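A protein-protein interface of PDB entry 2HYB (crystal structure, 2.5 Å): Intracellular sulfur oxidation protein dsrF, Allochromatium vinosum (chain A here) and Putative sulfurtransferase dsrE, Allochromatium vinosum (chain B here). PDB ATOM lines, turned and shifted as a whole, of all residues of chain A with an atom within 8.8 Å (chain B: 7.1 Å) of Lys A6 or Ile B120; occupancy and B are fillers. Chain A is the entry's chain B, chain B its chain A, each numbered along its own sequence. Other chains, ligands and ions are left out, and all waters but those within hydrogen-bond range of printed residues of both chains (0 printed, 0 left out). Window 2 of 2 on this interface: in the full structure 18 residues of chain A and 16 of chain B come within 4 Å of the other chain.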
ATOM      1  N   VAL A   5      13.811 -18.228 -26.085  1.00  0.00           N
ATOM      2  CA  VAL A   5      14.786 -18.282 -27.172  1.00  0.00           C
ATOM      3  C   VAL A   5      15.815 -17.158 -27.053  1.00  0.00           C
ATOM      4  O   VAL A   5      17.009 -17.421 -26.947  1.00  0.00           O
ATOM      5  CB  VAL A   5      14.091 -18.215 -28.559  1.00  0.00           C
ATOM      6  CG1 VAL A   5      15.097 -18.531 -29.646  1.00  0.00           C
ATOM      7  CG2 VAL A   5      12.930 -19.203 -28.611  1.00  0.00           C
ATOM      8  N   LYS A   6      15.347 -15.911 -27.066  1.00  0.00           N
ATOM      9  CA  LYS A   6      16.240 -14.751 -26.942  1.00  0.00           C
ATOM     10  C   LYS A   6      16.526 -14.351 -25.502  1.00  0.00           C
ATOM     11  O   LYS A   6      15.728 -14.601 -24.609  1.00  0.00           O
ATOM     12  CB  LYS A   6      15.669 -13.528 -27.669  1.00  0.00           C
ATOM     13  CG  LYS A   6      15.804 -13.549 -29.160  1.00  0.00           C
ATOM     14  CD  LYS A   6      15.324 -12.236 -29.737  1.00  0.00           C
ATOM     15  CE  LYS A   6      15.569 -12.156 -31.237  1.00  0.00           C
ATOM     16  NZ  LYS A   6      15.119 -10.843 -31.768  1.00  0.00           N
ATOM     17  N   LYS A   7      17.671 -13.715 -25.292  1.00  0.00           N
ATOM     18  CA  LYS A   7      18.068 -13.246 -23.965  1.00  0.00           C
ATOM     19  C   LYS A   7      17.795 -11.745 -23.916  1.00  0.00           C
ATOM     20  O   LYS A   7      18.277 -10.978 -24.762  1.00  0.00           O
ATOM     21  CB  LYS A   7      19.554 -13.520 -23.721  1.00  0.00           C
ATOM     22  CG  LYS A   7      20.073 -13.023 -22.383  1.00  0.00           C
ATOM     23  CD  LYS A   7      19.396 -13.712 -21.196  1.00  0.00           C
ATOM     24  CE  LYS A   7      19.962 -13.209 -19.864  1.00  0.00           C
ATOM     25  NZ  LYS A   7      19.418 -13.926 -18.664  1.00  0.00           N
ATOM     26  N   PHE A   8      16.998 -11.336 -22.934  1.00  0.00           N
ATOM     27  CA  PHE A   8      16.616  -9.939 -22.772  1.00  0.00           C
ATOM     28  C   PHE A   8      17.125  -9.311 -21.490  1.00  0.00           C
ATOM     29  O   PHE A   8      16.927  -9.844 -20.396  1.00  0.00           O
ATOM     30  CB  PHE A   8      15.091  -9.804 -22.771  1.00  0.00           C
ATOM     31  CG  PHE A   8      14.460  -9.884 -24.128  1.00  0.00           C
ATOM     32  CD1 PHE A   8      13.082  -9.999 -24.246  1.00  0.00           C
ATOM     33  CD2 PHE A   8      15.225  -9.830 -25.287  1.00  0.00           C
ATOM     34  CE1 PHE A   8      12.469 -10.061 -25.495  1.00  0.00           C
ATOM     35  CE2 PHE A   8      14.618  -9.891 -26.546  1.00  0.00           C
ATOM     36  CZ  PHE A   8      13.238 -10.006 -26.648  1.00  0.00           C
ATOM     37  N   MET A   9      17.754  -8.152 -21.624  1.00  0.00           N
ATOM     38  CA  MET A   9      18.253  -7.448 -20.454  1.00  0.00           C
ATOM     39  C   MET A   9      17.475  -6.159 -20.220  1.00  0.00           C
ATOM     40  O   MET A   9      17.277  -5.365 -21.142  1.00  0.00           O
ATOM     41  CB  MET A   9      19.745  -7.122 -20.598  1.00  0.00           C
ATOM     42  CG  MET A   9      20.288  -6.328 -19.408  1.00  0.00           C
ATOM     43  SD  MET A   9      21.975  -5.740 -19.587  1.00  0.00           S
ATOM     44  CE  MET A   9      22.805  -7.129 -18.969  1.00  0.00           C
ATOM     45  N   TYR A  10      17.026  -5.972 -18.984  1.00  0.00           N
ATOM     46  CA  TYR A  10      16.293  -4.778 -18.600  1.00  0.00           C
ATOM     47  C   TYR A  10      17.247  -3.938 -17.776  1.00  0.00           C
ATOM     48  O   TYR A  10      17.436  -4.180 -16.578  1.00  0.00           O
ATOM     49  CB  TYR A  10      15.048  -5.143 -17.780  1.00  0.00           C
ATOM     50  CG  TYR A  10      13.897  -5.654 -18.626  1.00  0.00           C
ATOM     51  CD1 TYR A  10      13.137  -4.783 -19.401  1.00  0.00           C
ATOM     52  CD2 TYR A  10      13.601  -7.019 -18.686  1.00  0.00           C
ATOM     53  CE1 TYR A  10      12.119  -5.257 -20.211  1.00  0.00           C
ATOM     54  CE2 TYR A  10      12.588  -7.500 -19.494  1.00  0.00           C
ATOM     55  CZ  TYR A  10      11.851  -6.618 -20.255  1.00  0.00           C
ATOM     56  OH  TYR A  10      10.852  -7.104 -21.067  1.00  0.00           O
ATOM     57  N   ILE A  31       4.998  -7.655 -18.038  1.00  0.00           N
ATOM     58  CA  ILE A  31       4.334  -7.990 -19.295  1.00  0.00           C
ATOM     59  C   ILE A  31       5.161  -8.906 -20.205  1.00  0.00           C
ATOM     60  O   ILE A  31       4.605  -9.736 -20.942  1.00  0.00           O
ATOM     61  CB  ILE A  31       3.962  -6.706 -20.068  1.00  0.00           C
ATOM     62  CG1 ILE A  31       2.770  -6.052 -19.384  1.00  0.00           C
ATOM     63  CG2 ILE A  31       3.611  -7.020 -21.514  1.00  0.00           C
ATOM     64  CD1 ILE A  31       1.565  -6.973 -19.295  1.00  0.00           C
ATOM     65  N   GLY A  32       6.482  -8.756 -20.155  1.00  0.00           N
ATOM     66  CA  GLY A  32       7.351  -9.574 -20.987  1.00  0.00           C
ATOM     67  C   GLY A  32       7.552 -10.965 -20.424  1.00  0.00           C
ATOM     68  O   GLY A  32       8.043 -11.858 -21.113  1.00  0.00           O
ATOM     69  N   ALA A  33       7.177 -11.148 -19.163  1.00  0.00           N
ATOM     70  CA  ALA A  33       7.315 -12.436 -18.499  1.00  0.00           C
ATOM     71  C   ALA A  33       6.497 -13.489 -19.238  1.00  0.00           C
ATOM     72  O   ALA A  33       6.927 -14.635 -19.397  1.00  0.00           O
ATOM     73  CB  ALA A  33       6.835 -12.325 -17.058  1.00  0.00           C
ATOM     74  N   ALA A  34       5.316 -13.073 -19.687  1.00  0.00           N
ATOM     75  CA  ALA A  34       4.376 -13.931 -20.396  1.00  0.00           C
ATOM     76  C   ALA A  34       4.870 -14.493 -21.726  1.00  0.00           C
ATOM     77  O   ALA A  34       4.311 -15.466 -22.235  1.00  0.00           O
ATOM     78  CB  ALA A  34       3.069 -13.177 -20.614  1.00  0.00           C
ATOM     79  N   PHE A  35       5.901 -13.887 -22.303  1.00  0.00           N
ATOM     80  CA  PHE A  35       6.430 -14.369 -23.574  1.00  0.00           C
ATOM     81  C   PHE A  35       7.586 -15.342 -23.357  1.00  0.00           C
ATOM     82  O   PHE A  35       8.243 -15.769 -24.309  1.00  0.00           O
ATOM     83  CB  PHE A  35       6.893 -13.198 -24.436  1.00  0.00           C
ATOM     84  CG  PHE A  35       5.782 -12.269 -24.853  1.00  0.00           C
ATOM     85  CD1 PHE A  35       5.208 -11.381 -23.940  1.00  0.00           C
ATOM     86  CD2 PHE A  35       5.315 -12.273 -26.172  1.00  0.00           C
ATOM     87  CE1 PHE A  35       4.186 -10.509 -24.336  1.00  0.00           C
ATOM     88  CE2 PHE A  35       4.289 -11.402 -26.575  1.00  0.00           C
ATOM     89  CZ  PHE A  35       3.727 -10.521 -25.655  1.00  0.00           C
ATOM     90  N   ASP A  36       7.814 -15.693 -22.093  1.00  0.00           N
ATOM     91  CA  ASP A  36       8.871 -16.617 -21.684  1.00  0.00           C
ATOM     92  C   ASP A  36      10.168 -16.592 -22.480  1.00  0.00           C
ATOM     93  O   ASP A  36      10.500 -17.549 -23.178  1.00  0.00           O
ATOM     94  CB  ASP A  36       8.331 -18.053 -21.625  1.00  0.00           C
ATOM     95  CG  ASP A  36       7.592 -18.456 -22.884  1.00  0.00           C
ATOM     96  OD1 ASP A  36       6.510 -17.889 -23.144  1.00  0.00           O
ATOM     97  OD2 ASP A  36       8.089 -19.338 -23.613  1.00  0.00           O
ATOM     98  N   GLN A  37      10.893 -15.485 -22.376  1.00  0.00           N
ATOM     99  CA  GLN A  37      12.181 -15.365 -23.036  1.00  0.00           C
ATOM    100  C   GLN A  37      13.153 -15.411 -21.868  1.00  0.00           C
ATOM    101  O   GLN A  37      12.749 -15.206 -20.722  1.00  0.00           O
ATOM    102  CB  GLN A  37      12.317 -14.021 -23.758  1.00  0.00           C
ATOM    103  CG  GLN A  37      11.325 -13.783 -24.878  1.00  0.00           C
ATOM    104  CD  GLN A  37      11.521 -14.717 -26.061  1.00  0.00           C
ATOM    105  OE1 GLN A  37      12.610 -14.805 -26.630  1.00  0.00           O
ATOM    106  NE2 GLN A  37      10.458 -15.409 -26.446  1.00  0.00           N
ATOM    107  N   ASP A  38      14.419 -15.701 -22.132  1.00  0.00           N
ATOM    108  CA  ASP A  38      15.376 -15.732 -21.042  1.00  0.00           C
ATOM    109  C   ASP A  38      15.556 -14.280 -20.613  1.00  0.00           C
ATOM    110  O   ASP A  38      16.302 -13.524 -21.237  1.00  0.00           O
ATOM    111  CB  ASP A  38      16.697 -16.324 -21.510  1.00  0.00           C
ATOM    112  CG  ASP A  38      17.557 -16.778 -20.357  1.00  0.00           C
ATOM    113  OD1 ASP A  38      17.495 -16.136 -19.284  1.00  0.00           O
ATOM    114  OD2 ASP A  38      18.304 -17.766 -20.524  1.00  0.00           O
ATOM    115  N   VAL A  39      14.850 -13.892 -19.556  1.00  0.00           N
ATOM    116  CA  VAL A  39      14.904 -12.522 -19.061  1.00  0.00           C
ATOM    117  C   VAL A  39      15.799 -12.335 -17.847  1.00  0.00           C
ATOM    118  O   VAL A  39      15.851 -13.189 -16.957  1.00  0.00           O
ATOM    119  CB  VAL A  39      13.481 -12.006 -18.686  1.00  0.00           C
ATOM    120  CG1 VAL A  39      13.568 -10.679 -17.929  1.00  0.00           C
ATOM    121  CG2 VAL A  39      12.643 -11.833 -19.944  1.00  0.00           C
ATOM    122  N   CYS A  40      16.501 -11.206 -17.821  1.00  0.00           N
ATOM    123  CA  CYS A  40      17.348 -10.857 -16.690  1.00  0.00           C
ATOM    124  C   CYS A  40      17.219  -9.357 -16.483  1.00  0.00           C
ATOM    125  O   CYS A  40      17.182  -8.582 -17.437  1.00  0.00           O
ATOM    126  CB  CYS A  40      18.808 -11.248 -16.933  1.00  0.00           C
ATOM    127  SG  CYS A  40      19.789 -10.078 -17.854  1.00  0.00           S
ATOM    128  N   GLU A 129      26.023 -11.006 -23.482  1.00  0.00           N
ATOM    129  CA  GLU A 129      25.219 -12.209 -23.674  1.00  0.00           C
ATOM    130  C   GLU A 129      23.797 -11.872 -24.108  1.00  0.00           C
ATOM    131  O   GLU A 129      23.114 -12.704 -24.699  1.00  0.00           O
ATOM    132  CB  GLU A 129      25.153 -13.017 -22.375  1.00  0.00           C
ATOM    133  CG  GLU A 129      26.306 -13.968 -22.127  1.00  0.00           C
ATOM    134  CD  GLU A 129      26.301 -14.491 -20.703  1.00  0.00           C
ATOM    135  OE1 GLU A 129      25.219 -14.882 -20.214  1.00  0.00           O
ATOM    136  OE2 GLU A 129      27.377 -14.520 -20.073  1.00  0.00           O
ATOM    137  N   SER A 130      23.349 -10.659 -23.805  1.00  0.00           N
ATOM    138  CA  SER A 130      21.995 -10.250 -24.153  1.00  0.00           C
ATOM    139  C   SER A 130      21.804 -10.035 -25.650  1.00  0.00           C
ATOM    140  O   SER A 130      22.697  -9.519 -26.325  1.00  0.00           O
ATOM    141  CB  SER A 130      21.631  -8.964 -23.414  1.00  0.00           C
ATOM    142  OG  SER A 130      21.838  -9.097 -22.019  1.00  0.00           O
ATOM    143  N   ASP A 131      20.639 -10.433 -26.160  1.00  0.00           N
ATOM    144  CA  ASP A 131      20.314 -10.269 -27.574  1.00  0.00           C
ATOM    145  C   ASP A 131      19.636  -8.915 -27.794  1.00  0.00           C
ATOM    146  O   ASP A 131      19.638  -8.370 -28.906  1.00  0.00           O
ATOM    147  CB  ASP A 131      19.361 -11.373 -28.038  1.00  0.00           C
ATOM    148  CG  ASP A 131      20.001 -12.742 -28.033  1.00  0.00           C
ATOM    149  OD1 ASP A 131      21.015 -12.933 -28.744  1.00  0.00           O
ATOM    150  OD2 ASP A 131      19.486 -13.628 -27.320  1.00  0.00           O
ATOM    151  N   ALA A 132      19.050  -8.385 -26.725  1.00  0.00           N
ATOM    152  CA  ALA A 132      18.365  -7.106 -26.789  1.00  0.00           C
ATOM    153  C   ALA A 132      18.312  -6.523 -25.399  1.00  0.00           C
ATOM    154  O   ALA A 132      18.142  -7.251 -24.422  1.00  0.00           O
ATOM    155  CB  ALA A 132      16.958  -7.287 -27.335  1.00  0.00           C
ATOM    156  N   PHE A 134      16.600  -3.356 -23.000  1.00  0.00           N
ATOM    157  CA  PHE A 134      15.585  -2.330 -22.821  1.00  0.00           C
ATOM    158  C   PHE A 134      16.236  -1.278 -21.933  1.00  0.00           C
ATOM    159  O   PHE A 134      16.883  -1.626 -20.944  1.00  0.00           O
ATOM    160  CB  PHE A 134      14.359  -2.935 -22.127  1.00  0.00           C
ATOM    161  CG  PHE A 134      13.614  -3.921 -22.979  1.00  0.00           C
ATOM    162  CD1 PHE A 134      12.816  -3.479 -24.026  1.00  0.00           C
ATOM    163  CD2 PHE A 134      13.739  -5.289 -22.766  1.00  0.00           C
ATOM    164  CE1 PHE A 134      12.154  -4.382 -24.849  1.00  0.00           C
ATOM    165  CE2 PHE A 134      13.078  -6.205 -23.588  1.00  0.00           C
ATOM    166  CZ  PHE A 134      12.286  -5.753 -24.630  1.00  0.00           C
ATOM    167  N   ALA B   4      13.183  -2.385 -34.406  1.00  0.00           N
ATOM    168  CA  ALA B   4      12.196  -2.126 -33.373  1.00  0.00           C
ATOM    169  C   ALA B   4      12.671  -0.887 -32.623  1.00  0.00           C
ATOM    170  O   ALA B   4      13.577  -0.961 -31.790  1.00  0.00           O
ATOM    171  CB  ALA B   4      12.104  -3.309 -32.424  1.00  0.00           C
ATOM    172  N   PHE B  35       9.990  -2.942 -38.093  1.00  0.00           N
ATOM    173  CA  PHE B  35       8.901  -3.802 -37.658  1.00  0.00           C
ATOM    174  C   PHE B  35       7.867  -3.036 -36.865  1.00  0.00           C
ATOM    175  O   PHE B  35       6.667  -3.238 -37.035  1.00  0.00           O
ATOM    176  CB  PHE B  35       9.427  -4.953 -36.798  1.00  0.00           C
ATOM    177  CG  PHE B  35       8.359  -5.913 -36.366  1.00  0.00           C
ATOM    178  CD1 PHE B  35       7.732  -6.741 -37.297  1.00  0.00           C
ATOM    179  CD2 PHE B  35       7.954  -5.971 -35.035  1.00  0.00           C
ATOM    180  CE1 PHE B  35       6.715  -7.614 -36.905  1.00  0.00           C
ATOM    181  CE2 PHE B  35       6.936  -6.841 -34.631  1.00  0.00           C
ATOM    182  CZ  PHE B  35       6.316  -7.663 -35.571  1.00  0.00           C
ATOM    183  N   LEU B 115       5.338  -4.086 -27.286  1.00  0.00           N
ATOM    184  CA  LEU B 115       6.712  -3.628 -27.222  1.00  0.00           C
ATOM    185  C   LEU B 115       7.570  -4.892 -27.185  1.00  0.00           C
ATOM    186  O   LEU B 115       8.426  -5.100 -28.052  1.00  0.00           O
ATOM    187  CB  LEU B 115       6.952  -2.785 -25.961  1.00  0.00           C
ATOM    188  CG  LEU B 115       8.426  -2.460 -25.672  1.00  0.00           C
ATOM    189  CD1 LEU B 115       9.041  -1.754 -26.869  1.00  0.00           C
ATOM    190  CD2 LEU B 115       8.549  -1.610 -24.431  1.00  0.00           C
ATOM    191  N   VAL B 116       7.326  -5.744 -26.191  1.00  0.00           N
ATOM    192  CA  VAL B 116       8.078  -6.983 -26.038  1.00  0.00           C
ATOM    193  C   VAL B 116       8.023  -7.824 -27.327  1.00  0.00           C
ATOM    194  O   VAL B 116       9.029  -8.388 -27.783  1.00  0.00           O
ATOM    195  CB  VAL B 116       7.526  -7.792 -24.845  1.00  0.00           C
ATOM    196  CG1 VAL B 116       8.229  -9.142 -24.763  1.00  0.00           C
ATOM    197  CG2 VAL B 116       7.726  -7.003 -23.552  1.00  0.00           C
ATOM    198  N   GLU B 117       6.829  -7.879 -27.902  1.00  0.00           N
ATOM    199  CA  GLU B 117       6.542  -8.602 -29.136  1.00  0.00           C
ATOM    200  C   GLU B 117       7.552  -8.210 -30.239  1.00  0.00           C
ATOM    201  O   GLU B 117       8.147  -9.069 -30.898  1.00  0.00           O
ATOM    202  CB  GLU B 117       5.111  -8.243 -29.563  1.00  0.00           C
ATOM    203  CG  GLU B 117       4.259  -9.368 -30.118  1.00  0.00           C
ATOM    204  CD  GLU B 117       4.687  -9.785 -31.497  1.00  0.00           C
ATOM    205  OE1 GLU B 117       5.774 -10.385 -31.620  1.00  0.00           O
ATOM    206  OE2 GLU B 117       3.937  -9.501 -32.457  1.00  0.00           O
ATOM    207  N   ALA B 118       7.731  -6.905 -30.434  1.00  0.00           N
ATOM    208  CA  ALA B 118       8.638  -6.373 -31.443  1.00  0.00           C
ATOM    209  C   ALA B 118      10.082  -6.721 -31.115  1.00  0.00           C
ATOM    210  O   ALA B 118      10.881  -7.029 -32.012  1.00  0.00           O
ATOM    211  CB  ALA B 118       8.479  -4.866 -31.537  1.00  0.00           C
ATOM    212  N   ALA B 119      10.416  -6.665 -29.828  1.00  0.00           N
ATOM    213  CA  ALA B 119      11.761  -6.991 -29.370  1.00  0.00           C
ATOM    214  C   ALA B 119      12.152  -8.387 -29.854  1.00  0.00           C
ATOM    215  O   ALA B 119      13.309  -8.651 -30.199  1.00  0.00           O
ATOM    216  CB  ALA B 119      11.817  -6.927 -27.854  1.00  0.00           C
ATOM    217  N   ILE B 120      11.166  -9.275 -29.894  1.00  0.00           N
ATOM    218  CA  ILE B 120      11.395 -10.642 -30.332  1.00  0.00           C
ATOM    219  C   ILE B 120      11.441 -10.764 -31.858  1.00  0.00           C
ATOM    220  O   ILE B 120      12.320 -11.430 -32.409  1.00  0.00           O
ATOM    221  CB  ILE B 120      10.313 -11.573 -29.772  1.00  0.00           C
ATOM    222  CG1 ILE B 120      10.297 -11.470 -28.243  1.00  0.00           C
ATOM    223  CG2 ILE B 120      10.574 -13.002 -30.218  1.00  0.00           C
ATOM    224  CD1 ILE B 120       9.295 -12.381 -27.556  1.00  0.00           C
ATOM    225  N   GLN B 121      10.505 -10.111 -32.539  1.00  0.00           N
ATOM    226  CA  GLN B 121      10.453 -10.153 -34.003  1.00  0.00           C
ATOM    227  C   GLN B 121      11.555  -9.385 -34.746  1.00  0.00           C
ATOM    228  O   GLN B 121      11.943  -9.773 -35.851  1.00  0.00           O
ATOM    229  CB  GLN B 121       9.095  -9.643 -34.502  1.00  0.00           C
ATOM    230  CG  GLN B 121       7.918 -10.482 -34.072  1.00  0.00           C
ATOM    231  CD  GLN B 121       8.089 -11.933 -34.459  1.00  0.00           C
ATOM    232  OE1 GLN B 121       8.144 -12.272 -35.643  1.00  0.00           O
ATOM    233  NE2 GLN B 121       8.188 -12.802 -33.458  1.00  0.00           N
ATOM    234  N   ALA B 122      12.039  -8.289 -34.168  1.00  0.00           N
ATOM    235  CA  ALA B 122      13.067  -7.501 -34.841  1.00  0.00           C
ATOM    236  C   ALA B 122      14.468  -7.997 -34.515  1.00  0.00           C
ATOM    237  O   ALA B 122      14.694  -8.631 -33.486  1.00  0.00           O
ATOM    238  CB  ALA B 122      12.930  -6.014 -34.471  1.00  0.00           C
ATOM    239  N   ASP B 123      15.406  -7.713 -35.411  1.00  0.00           N
ATOM    240  CA  ASP B 123      16.790  -8.120 -35.219  1.00  0.00           C
ATOM    241  C   ASP B 123      17.488  -7.157 -34.259  1.00  0.00           C
ATOM    242  O   ASP B 123      18.395  -7.540 -33.512  1.00  0.00           O
ATOM    243  CB  ASP B 123      17.523  -8.124 -36.561  1.00  0.00           C
ATOM    244  CG  ASP B 123      16.902  -9.073 -37.566  1.00  0.00           C
ATOM    245  OD1 ASP B 123      16.831 -10.285 -37.284  1.00  0.00           O
ATOM    246  OD2 ASP B 123      16.492  -8.605 -38.644  1.00  0.00           O
ATOM    247  N   ARG B 124      17.049  -5.903 -34.283  1.00  0.00           N
ATOM    248  CA  ARG B 124      17.636  -4.880 -33.439  1.00  0.00           C
ATOM    249  C   ARG B 124      16.605  -4.014 -32.728  1.00  0.00           C
ATOM    250  O   ARG B 124      15.624  -3.563 -33.323  1.00  0.00           O
ATOM    251  CB  ARG B 124      18.543  -3.974 -34.276  1.00  0.00           C
ATOM    252  CG  ARG B 124      19.712  -4.684 -34.934  1.00  0.00           C
ATOM    253  CD  ARG B 124      20.727  -5.170 -33.907  1.00  0.00           C
ATOM    254  NE  ARG B 124      21.903  -5.757 -34.548  1.00  0.00           N
ATOM    255  CZ  ARG B 124      21.887  -6.886 -35.248  1.00  0.00           C
ATOM    256  NH1 ARG B 124      20.756  -7.562 -35.397  1.00  0.00           N
ATOM    257  NH2 ARG B 124      22.996  -7.335 -35.813  1.00  0.00           N
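The backbone carbonyl oxygen (O) of Ala B119 lies within hydrogen-bond range of the side-chain amino group (NZ) of Lys A6, 3.2 Å away. O of Ala B122 lies within hydrogen-bond range of NZ of Lys A6 (2.8 Å). The backbone carbonyl oxygen (O) of Ile B120 lies within hydrogen-bond range of the side-chain amino group (NZ) of Lys A6 (2.9 Å).
The backbone NH (N) of Asp A38 is in hydrogen-bond range of the backbone carbonyl oxygen (O) of Lys A6 (3.0 Å). NE2 of Gln A37 lies within hydrogen-bond range of O of Phe A35 (3.1 Å). The backbone NH of Phe A134 is in hydrogen-bond range of the backbone carbonyl oxygen of Met A9. The backbone NH (N) of Tyr A10 is in hydrogen-bond range of the backbone carbonyl oxygen (O) of Cys A40. The side-chain amide oxygen of Gln A37 lies within hydrogen-bond range of the backbone NH of Lys A6 (3.0 Å). The backbone NH (N) of Phe A8 is in hydrogen-bond range of the backbone carbonyl oxygen (O) of Asp A38 (2.9 Å).
Phe A8 touches Ala B119 (CZ to CB, 3.6 Å). Phe A8 touches Ile B120 (CZ to CG1, 3.7 Å). Val B116 touches Tyr A10 (CG2 to OH, 3.99 Å). Val B116 touches Gly A32. Val B116 touches Phe A35 (CG1 to CD1, 3.8 Å). Ile B120 touches Gln A37 (CD1 to NE2, 3.4 Å). CZ of Phe A134 touches CB of Ala B119 (3.5 Å).
Lys A6 touches three residues of chain B. Of the printed residues of chain A, Ile B120 touches Lys A6, Phe A8 and Gln A37. Of the printed residues of chain B, Tyr A10 touches Val B116. Of the printed residues of chain B, Phe A35 touches Val B116 (3.8 Å). Of the printed residues of chain B, Phe A8 touches Ala B119 (3.6 Å) and Ile B120 (3.7 Å). The nearest residue of chain A that does not touch Ile B120 is Phe A35 (4.02 Å). The nearest printed residue of chain A that does not touch Ala B122 is Ala A132 (6.7 Å).
Of the 12 printed residues of chain B, 4 touch a printed residue of chain A. Hydrophobic or aromatic side chains of chain B that line the printed part of chain A: Val B116, Ala B119 and Ile B120. Among the printed residues, 10 pairs touch across the chains.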
